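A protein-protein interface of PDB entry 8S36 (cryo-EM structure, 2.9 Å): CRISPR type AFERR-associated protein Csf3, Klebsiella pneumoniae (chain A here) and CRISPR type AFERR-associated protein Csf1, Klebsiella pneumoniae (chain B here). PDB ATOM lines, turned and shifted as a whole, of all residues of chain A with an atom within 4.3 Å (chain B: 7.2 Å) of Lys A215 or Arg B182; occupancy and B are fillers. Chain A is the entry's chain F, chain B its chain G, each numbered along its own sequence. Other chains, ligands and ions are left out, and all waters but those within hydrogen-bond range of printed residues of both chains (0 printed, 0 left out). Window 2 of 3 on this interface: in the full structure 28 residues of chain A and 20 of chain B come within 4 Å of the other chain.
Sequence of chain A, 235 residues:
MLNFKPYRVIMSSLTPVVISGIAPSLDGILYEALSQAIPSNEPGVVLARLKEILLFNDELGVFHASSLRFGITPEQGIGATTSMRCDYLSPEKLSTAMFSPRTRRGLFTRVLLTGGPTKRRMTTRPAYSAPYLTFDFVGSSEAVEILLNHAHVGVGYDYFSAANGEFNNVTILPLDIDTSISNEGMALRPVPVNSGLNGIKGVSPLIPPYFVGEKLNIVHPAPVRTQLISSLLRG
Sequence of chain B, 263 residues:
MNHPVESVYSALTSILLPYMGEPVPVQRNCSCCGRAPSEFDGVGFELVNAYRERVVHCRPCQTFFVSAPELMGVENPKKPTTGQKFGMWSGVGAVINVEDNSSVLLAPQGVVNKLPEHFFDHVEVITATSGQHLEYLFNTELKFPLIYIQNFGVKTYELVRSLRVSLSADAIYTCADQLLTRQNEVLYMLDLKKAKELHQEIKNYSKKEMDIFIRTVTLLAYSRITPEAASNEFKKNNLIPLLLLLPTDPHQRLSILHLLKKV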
ATOM      1  N   ILE A  19      18.122   0.967   0.538  1.00  0.00           N
ATOM      2  CA  ILE A  19      18.067   0.327   1.851  1.00  0.00           C
ATOM      3  C   ILE A  19      19.126  -0.767   1.907  1.00  0.00           C
ATOM      4  O   ILE A  19      19.129  -1.682   1.077  1.00  0.00           O
ATOM      5  CB  ILE A  19      16.671  -0.246   2.137  1.00  0.00           C
ATOM      6  CG1 ILE A  19      15.597   0.832   1.978  1.00  0.00           C
ATOM      7  CG2 ILE A  19      16.622  -0.846   3.534  1.00  0.00           C
ATOM      8  CD1 ILE A  19      15.583   1.872   3.060  1.00  0.00           C
ATOM      9  N   SER A  20      20.021  -0.677   2.889  1.00  0.00           N
ATOM     10  CA  SER A  20      21.120  -1.633   3.029  1.00  0.00           C
ATOM     11  C   SER A  20      20.691  -2.853   3.848  1.00  0.00           C
ATOM     12  O   SER A  20      21.301  -3.216   4.853  1.00  0.00           O
ATOM     13  CB  SER A  20      22.334  -0.950   3.649  1.00  0.00           C
ATOM     14  OG  SER A  20      21.998  -0.329   4.877  1.00  0.00           O
ATOM     15  N   GLY A  21      19.613  -3.486   3.396  1.00  0.00           N
ATOM     16  CA  GLY A  21      19.157  -4.718   4.005  1.00  0.00           C
ATOM     17  C   GLY A  21      18.323  -4.449   5.236  1.00  0.00           C
ATOM     18  O   GLY A  21      17.119  -4.714   5.255  1.00  0.00           O
ATOM     19  N   ILE A  22      18.963  -3.919   6.269  1.00  0.00           N
ATOM     20  CA  ILE A  22      18.248  -3.426   7.438  1.00  0.00           C
ATOM     21  C   ILE A  22      17.770  -2.015   7.139  1.00  0.00           C
ATOM     22  O   ILE A  22      18.467  -1.236   6.477  1.00  0.00           O
ATOM     23  CB  ILE A  22      19.149  -3.457   8.685  1.00  0.00           C
ATOM     24  CG1 ILE A  22      19.937  -4.771   8.764  1.00  0.00           C
ATOM     25  CG2 ILE A  22      18.320  -3.249   9.944  1.00  0.00           C
ATOM     26  CD1 ILE A  22      19.091  -6.021   8.634  1.00  0.00           C
ATOM     27  N   VAL A 203      21.696  -9.955  11.558  1.00  0.00           N
ATOM     28  CA  VAL A 203      22.991  -9.781  12.210  1.00  0.00           C
ATOM     29  C   VAL A 203      23.427  -8.340  12.001  1.00  0.00           C
ATOM     30  O   VAL A 203      23.598  -7.898  10.858  1.00  0.00           O
ATOM     31  CB  VAL A 203      24.040 -10.759  11.659  1.00  0.00           C
ATOM     32  CG1 VAL A 203      25.427 -10.387  12.154  1.00  0.00           C
ATOM     33  CG2 VAL A 203      23.690 -12.186  12.057  1.00  0.00           C
ATOM     34  N   SER A 204      23.605  -7.609  13.094  1.00  0.00           N
ATOM     35  CA  SER A 204      23.924  -6.190  13.024  1.00  0.00           C
ATOM     36  C   SER A 204      24.329  -5.713  14.418  1.00  0.00           C
ATOM     37  O   SER A 204      23.987  -6.358  15.415  1.00  0.00           O
ATOM     38  CB  SER A 204      22.732  -5.373  12.506  1.00  0.00           C
ATOM     39  OG  SER A 204      22.915  -3.990  12.754  1.00  0.00           O
ATOM     40  N   PRO A 205      25.114  -4.637  14.506  1.00  0.00           N
ATOM     41  CA  PRO A 205      25.245  -3.942  15.789  1.00  0.00           C
ATOM     42  C   PRO A 205      23.981  -3.164  16.110  1.00  0.00           C
ATOM     43  O   PRO A 205      23.223  -2.772  15.219  1.00  0.00           O
ATOM     44  CB  PRO A 205      26.441  -3.003  15.579  1.00  0.00           C
ATOM     45  CG  PRO A 205      26.955  -3.270  14.196  1.00  0.00           C
ATOM     46  CD  PRO A 205      25.876  -3.963  13.444  1.00  0.00           C
ATOM     47  N   TYR A 210      26.317   1.505  12.092  1.00  0.00           N
ATOM     48  CA  TYR A 210      25.871   0.125  11.980  1.00  0.00           C
ATOM     49  C   TYR A 210      26.800  -0.738  11.140  1.00  0.00           C
ATOM     50  O   TYR A 210      26.403  -1.839  10.745  1.00  0.00           O
ATOM     51  CB  TYR A 210      24.463   0.088  11.384  1.00  0.00           C
ATOM     52  CG  TYR A 210      23.381   0.533  12.337  1.00  0.00           C
ATOM     53  CD1 TYR A 210      22.908  -0.322  13.320  1.00  0.00           C
ATOM     54  CD2 TYR A 210      22.830   1.801  12.250  1.00  0.00           C
ATOM     55  CE1 TYR A 210      21.919   0.076  14.192  1.00  0.00           C
ATOM     56  CE2 TYR A 210      21.839   2.209  13.119  1.00  0.00           C
ATOM     57  CZ  TYR A 210      21.387   1.341  14.087  1.00  0.00           C
ATOM     58  OH  TYR A 210      20.399   1.737  14.958  1.00  0.00           O
ATOM     59  N   GLY A 213      31.955  -2.609  14.985  1.00  0.00           N
ATOM     60  CA  GLY A 213      31.660  -3.376  16.175  1.00  0.00           C
ATOM     61  C   GLY A 213      31.153  -4.761  15.845  1.00  0.00           C
ATOM     62  O   GLY A 213      30.841  -5.059  14.688  1.00  0.00           O
ATOM     63  N   GLU A 214      31.068  -5.617  16.856  1.00  0.00           N
ATOM     64  CA  GLU A 214      30.542  -6.957  16.648  1.00  0.00           C
ATOM     65  C   GLU A 214      29.087  -6.888  16.199  1.00  0.00           C
ATOM     66  O   GLU A 214      28.283  -6.123  16.742  1.00  0.00           O
ATOM     67  CB  GLU A 214      30.682  -7.793  17.926  1.00  0.00           C
ATOM     68  CG  GLU A 214      30.107  -7.170  19.207  1.00  0.00           C
ATOM     69  CD  GLU A 214      28.607  -7.343  19.331  1.00  0.00           C
ATOM     70  OE1 GLU A 214      28.057  -8.238  18.660  1.00  0.00           O
ATOM     71  OE2 GLU A 214      27.979  -6.582  20.097  1.00  0.00           O
ATOM     72  N   LYS A 215      28.758  -7.681  15.184  1.00  0.00           N
ATOM     73  CA  LYS A 215      27.411  -7.733  14.615  1.00  0.00           C
ATOM     74  C   LYS A 215      26.669  -8.882  15.282  1.00  0.00           C
ATOM     75  O   LYS A 215      26.900 -10.051  14.965  1.00  0.00           O
ATOM     76  CB  LYS A 215      27.464  -7.915  13.101  1.00  0.00           C
ATOM     77  CG  LYS A 215      28.361  -6.925  12.367  1.00  0.00           C
ATOM     78  CD  LYS A 215      28.556  -7.319  10.908  1.00  0.00           C
ATOM     79  CE  LYS A 215      27.299  -7.091  10.076  1.00  0.00           C
ATOM     80  NZ  LYS A 215      26.950  -5.649   9.953  1.00  0.00           N
ATOM     81  N   LEU A 216      25.778  -8.559  16.215  1.00  0.00           N
ATOM     82  CA  LEU A 216      25.093  -9.577  16.998  1.00  0.00           C
ATOM     83  C   LEU A 216      23.708  -9.844  16.426  1.00  0.00           C
ATOM     84  O   LEU A 216      23.205  -9.112  15.569  1.00  0.00           O
ATOM     85  CB  LEU A 216      24.982  -9.169  18.473  1.00  0.00           C
ATOM     86  CG  LEU A 216      24.214  -7.896  18.839  1.00  0.00           C
ATOM     87  CD1 LEU A 216      23.734  -7.997  20.279  1.00  0.00           C
ATOM     88  CD2 LEU A 216      25.060  -6.645  18.651  1.00  0.00           C
ATOM     89  N   ARG B 164      25.575 -17.252  -1.342  1.00  0.00           N
ATOM     90  CA  ARG B 164      24.930 -17.368  -0.042  1.00  0.00           C
ATOM     91  C   ARG B 164      24.114 -18.650  -0.014  1.00  0.00           C
ATOM     92  O   ARG B 164      23.369 -18.934  -0.956  1.00  0.00           O
ATOM     93  CB  ARG B 164      24.028 -16.166   0.247  1.00  0.00           C
ATOM     94  CG  ARG B 164      24.774 -14.858   0.416  1.00  0.00           C
ATOM     95  CD  ARG B 164      25.508 -14.792   1.742  1.00  0.00           C
ATOM     96  NE  ARG B 164      26.035 -13.458   2.000  1.00  0.00           N
ATOM     97  CZ  ARG B 164      27.068 -12.920   1.364  1.00  0.00           C
ATOM     98  NH1 ARG B 164      27.725 -13.581   0.423  1.00  0.00           N
ATOM     99  NH2 ARG B 164      27.453 -11.687   1.680  1.00  0.00           N
ATOM    100  N   LEU B 179      27.876  -8.601  -7.479  1.00  0.00           N
ATOM    101  CA  LEU B 179      28.337  -8.597  -6.096  1.00  0.00           C
ATOM    102  C   LEU B 179      27.153  -8.435  -5.155  1.00  0.00           C
ATOM    103  O   LEU B 179      26.404  -7.458  -5.244  1.00  0.00           O
ATOM    104  CB  LEU B 179      29.350  -7.472  -5.886  1.00  0.00           C
ATOM    105  CG  LEU B 179      30.079  -7.455  -4.542  1.00  0.00           C
ATOM    106  CD1 LEU B 179      30.961  -8.683  -4.381  1.00  0.00           C
ATOM    107  CD2 LEU B 179      30.901  -6.183  -4.401  1.00  0.00           C
ATOM    108  N   LEU B 180      26.991  -9.401  -4.252  1.00  0.00           N
ATOM    109  CA  LEU B 180      25.832  -9.449  -3.364  1.00  0.00           C
ATOM    110  C   LEU B 180      26.121  -8.623  -2.117  1.00  0.00           C
ATOM    111  O   LEU B 180      26.381  -9.142  -1.029  1.00  0.00           O
ATOM    112  CB  LEU B 180      25.483 -10.888  -3.012  1.00  0.00           C
ATOM    113  CG  LEU B 180      24.147 -11.090  -2.292  1.00  0.00           C
ATOM    114  CD1 LEU B 180      22.981 -10.681  -3.174  1.00  0.00           C
ATOM    115  CD2 LEU B 180      24.004 -12.533  -1.860  1.00  0.00           C
ATOM    116  N   THR B 181      26.071  -7.308  -2.283  1.00  0.00           N
ATOM    117  CA  THR B 181      26.122  -6.441  -1.122  1.00  0.00           C
ATOM    118  C   THR B 181      24.779  -6.483  -0.405  1.00  0.00           C
ATOM    119  O   THR B 181      23.771  -6.945  -0.945  1.00  0.00           O
ATOM    120  CB  THR B 181      26.456  -5.007  -1.531  1.00  0.00           C
ATOM    121  OG1 THR B 181      25.675  -4.639  -2.676  1.00  0.00           O
ATOM    122  CG2 THR B 181      27.934  -4.876  -1.866  1.00  0.00           C
ATOM    123  N   ARG B 182      24.766  -5.994   0.834  1.00  0.00           N
ATOM    124  CA  ARG B 182      23.518  -5.974   1.582  1.00  0.00           C
ATOM    125  C   ARG B 182      22.499  -5.014   0.985  1.00  0.00           C
ATOM    126  O   ARG B 182      21.330  -5.048   1.382  1.00  0.00           O
ATOM    127  CB  ARG B 182      23.784  -5.595   3.037  1.00  0.00           C
ATOM    128  CG  ARG B 182      22.736  -6.114   4.000  1.00  0.00           C
ATOM    129  CD  ARG B 182      23.029  -7.541   4.427  1.00  0.00           C
ATOM    130  NE  ARG B 182      23.960  -7.593   5.548  1.00  0.00           N
ATOM    131  CZ  ARG B 182      23.657  -7.257   6.794  1.00  0.00           C
ATOM    132  NH1 ARG B 182      22.450  -6.825   7.123  1.00  0.00           N
ATOM    133  NH2 ARG B 182      24.591  -7.354   7.737  1.00  0.00           N
ATOM    134  N   GLN B 183      22.912  -4.167   0.045  1.00  0.00           N
ATOM    135  CA  GLN B 183      22.035  -3.183  -0.564  1.00  0.00           C
ATOM    136  C   GLN B 183      21.268  -3.717  -1.761  1.00  0.00           C
ATOM    137  O   GLN B 183      20.254  -3.122  -2.145  1.00  0.00           O
ATOM    138  CB  GLN B 183      22.851  -1.972  -1.003  1.00  0.00           C
ATOM    139  CG  GLN B 183      23.455  -1.211   0.146  1.00  0.00           C
ATOM    140  CD  GLN B 183      24.685  -1.869   0.732  1.00  0.00           C
ATOM    141  OE1 GLN B 183      24.695  -2.272   1.894  1.00  0.00           O
ATOM    142  NE2 GLN B 183      25.739  -1.971  -0.069  1.00  0.00           N
ATOM    143  N   ASN B 184      21.724  -4.817  -2.357  1.00  0.00           N
ATOM    144  CA  ASN B 184      21.095  -5.385  -3.541  1.00  0.00           C
ATOM    145  C   ASN B 184      20.713  -6.842  -3.344  1.00  0.00           C
ATOM    146  O   ASN B 184      20.385  -7.524  -4.322  1.00  0.00           O
ATOM    147  CB  ASN B 184      22.015  -5.240  -4.757  1.00  0.00           C
ATOM    148  CG  ASN B 184      23.399  -5.806  -4.513  1.00  0.00           C
ATOM    149  OD1 ASN B 184      23.620  -6.556  -3.564  1.00  0.00           O
ATOM    150  ND2 ASN B 184      24.344  -5.447  -5.374  1.00  0.00           N
ATOM    151  N   GLU B 185      20.734  -7.336  -2.108  1.00  0.00           N
ATOM    152  CA  GLU B 185      20.264  -8.688  -1.856  1.00  0.00           C
ATOM    153  C   GLU B 185      18.752  -8.798  -1.952  1.00  0.00           C
ATOM    154  O   GLU B 185      18.238  -9.917  -2.038  1.00  0.00           O
ATOM    155  CB  GLU B 185      20.733  -9.151  -0.476  1.00  0.00           C
ATOM    156  CG  GLU B 185      20.149  -8.354   0.682  1.00  0.00           C
ATOM    157  CD  GLU B 185      20.778  -8.710   2.015  1.00  0.00           C
ATOM    158  OE1 GLU B 185      21.904  -9.251   2.019  1.00  0.00           O
ATOM    159  OE2 GLU B 185      20.148  -8.446   3.060  1.00  0.00           O
ATOM    160  N   VAL B 186      18.032  -7.675  -1.971  1.00  0.00           N
ATOM    161  CA  VAL B 186      16.582  -7.729  -2.144  1.00  0.00           C
ATOM    162  C   VAL B 186      16.235  -8.135  -3.570  1.00  0.00           C
ATOM    163  O   VAL B 186      15.248  -8.841  -3.806  1.00  0.00           O
ATOM    164  CB  VAL B 186      15.943  -6.380  -1.765  1.00  0.00           C
ATOM    165  CG1 VAL B 186      16.412  -5.267  -2.697  1.00  0.00           C
ATOM    166  CG2 VAL B 186      14.428  -6.493  -1.784  1.00  0.00           C
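Of the printed residues of chain B, Ile A19 touches Gln B183 (3.7 Å).
Of the printed residues of chain B, Ser A20 touches Arg B182 (3.3 Å) and Gln B183 (3.2 Å).
Of the printed residues of chain B, Ile A22 touches Arg B182 (3.6 Å).
Printed residues of chain B within 4 Å of Val A203: Arg B182 (3.3 Å).
Pro A205 touches none of the printed residues of chain B.
Glu A214 touches none of the printed residues of chain B.
Lys A215 touches just one residue of chain B: Arg B182.
Printed residues of chain A within 4 Å of Arg B182: Ser A20 (3.3 Å), Gly A21 (3.1 Å), Ile A22 (3.6 Å), Val A203 (3.3 Å) and Lys A215 (3.6 Å).
The nearest printed residue of chain B that does not touch Gly A21 is Gln B183 (4.7 Å).
Ile A19 touches Gln B183.
Ser A20 touches Arg B182.
Ser A20 touches Gln B183.
Gly A21 touches Glu B185.
CG1 of Ile A22 touches NH1 of Arg B182, 3.6 Å away.
Lys A215 touches Arg B182.
Printed residues of chain A that touch a printed residue of chain B: Ile A19, Ser A20, Gly A21, Ile A22, Val A203 and Lys A215.
Hydrophobic or aromatic side chains of chain A within 4 Å of the printed part of chain B: Ile A22.
Of the 9 printed residues of chain B, 3 touch a printed residue of chain A.
Along chain B the printed residues that touch a printed residue of chain A span positions 182 to 185.
Among the printed residues, no Asp or Glu carboxylate lies within 4 Å of a Lys or Arg side-chain nitrogen of the other chain.
The backbone NH (N) of Gly A21 lies within hydrogen-bond range of the backbone carbonyl oxygen (O) of Arg B182, at 3.1 Å.
The guanidinium group (NH2) of Arg B182 lies within hydrogen-bond range of the backbone carbonyl oxygen (O) of Val A203.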
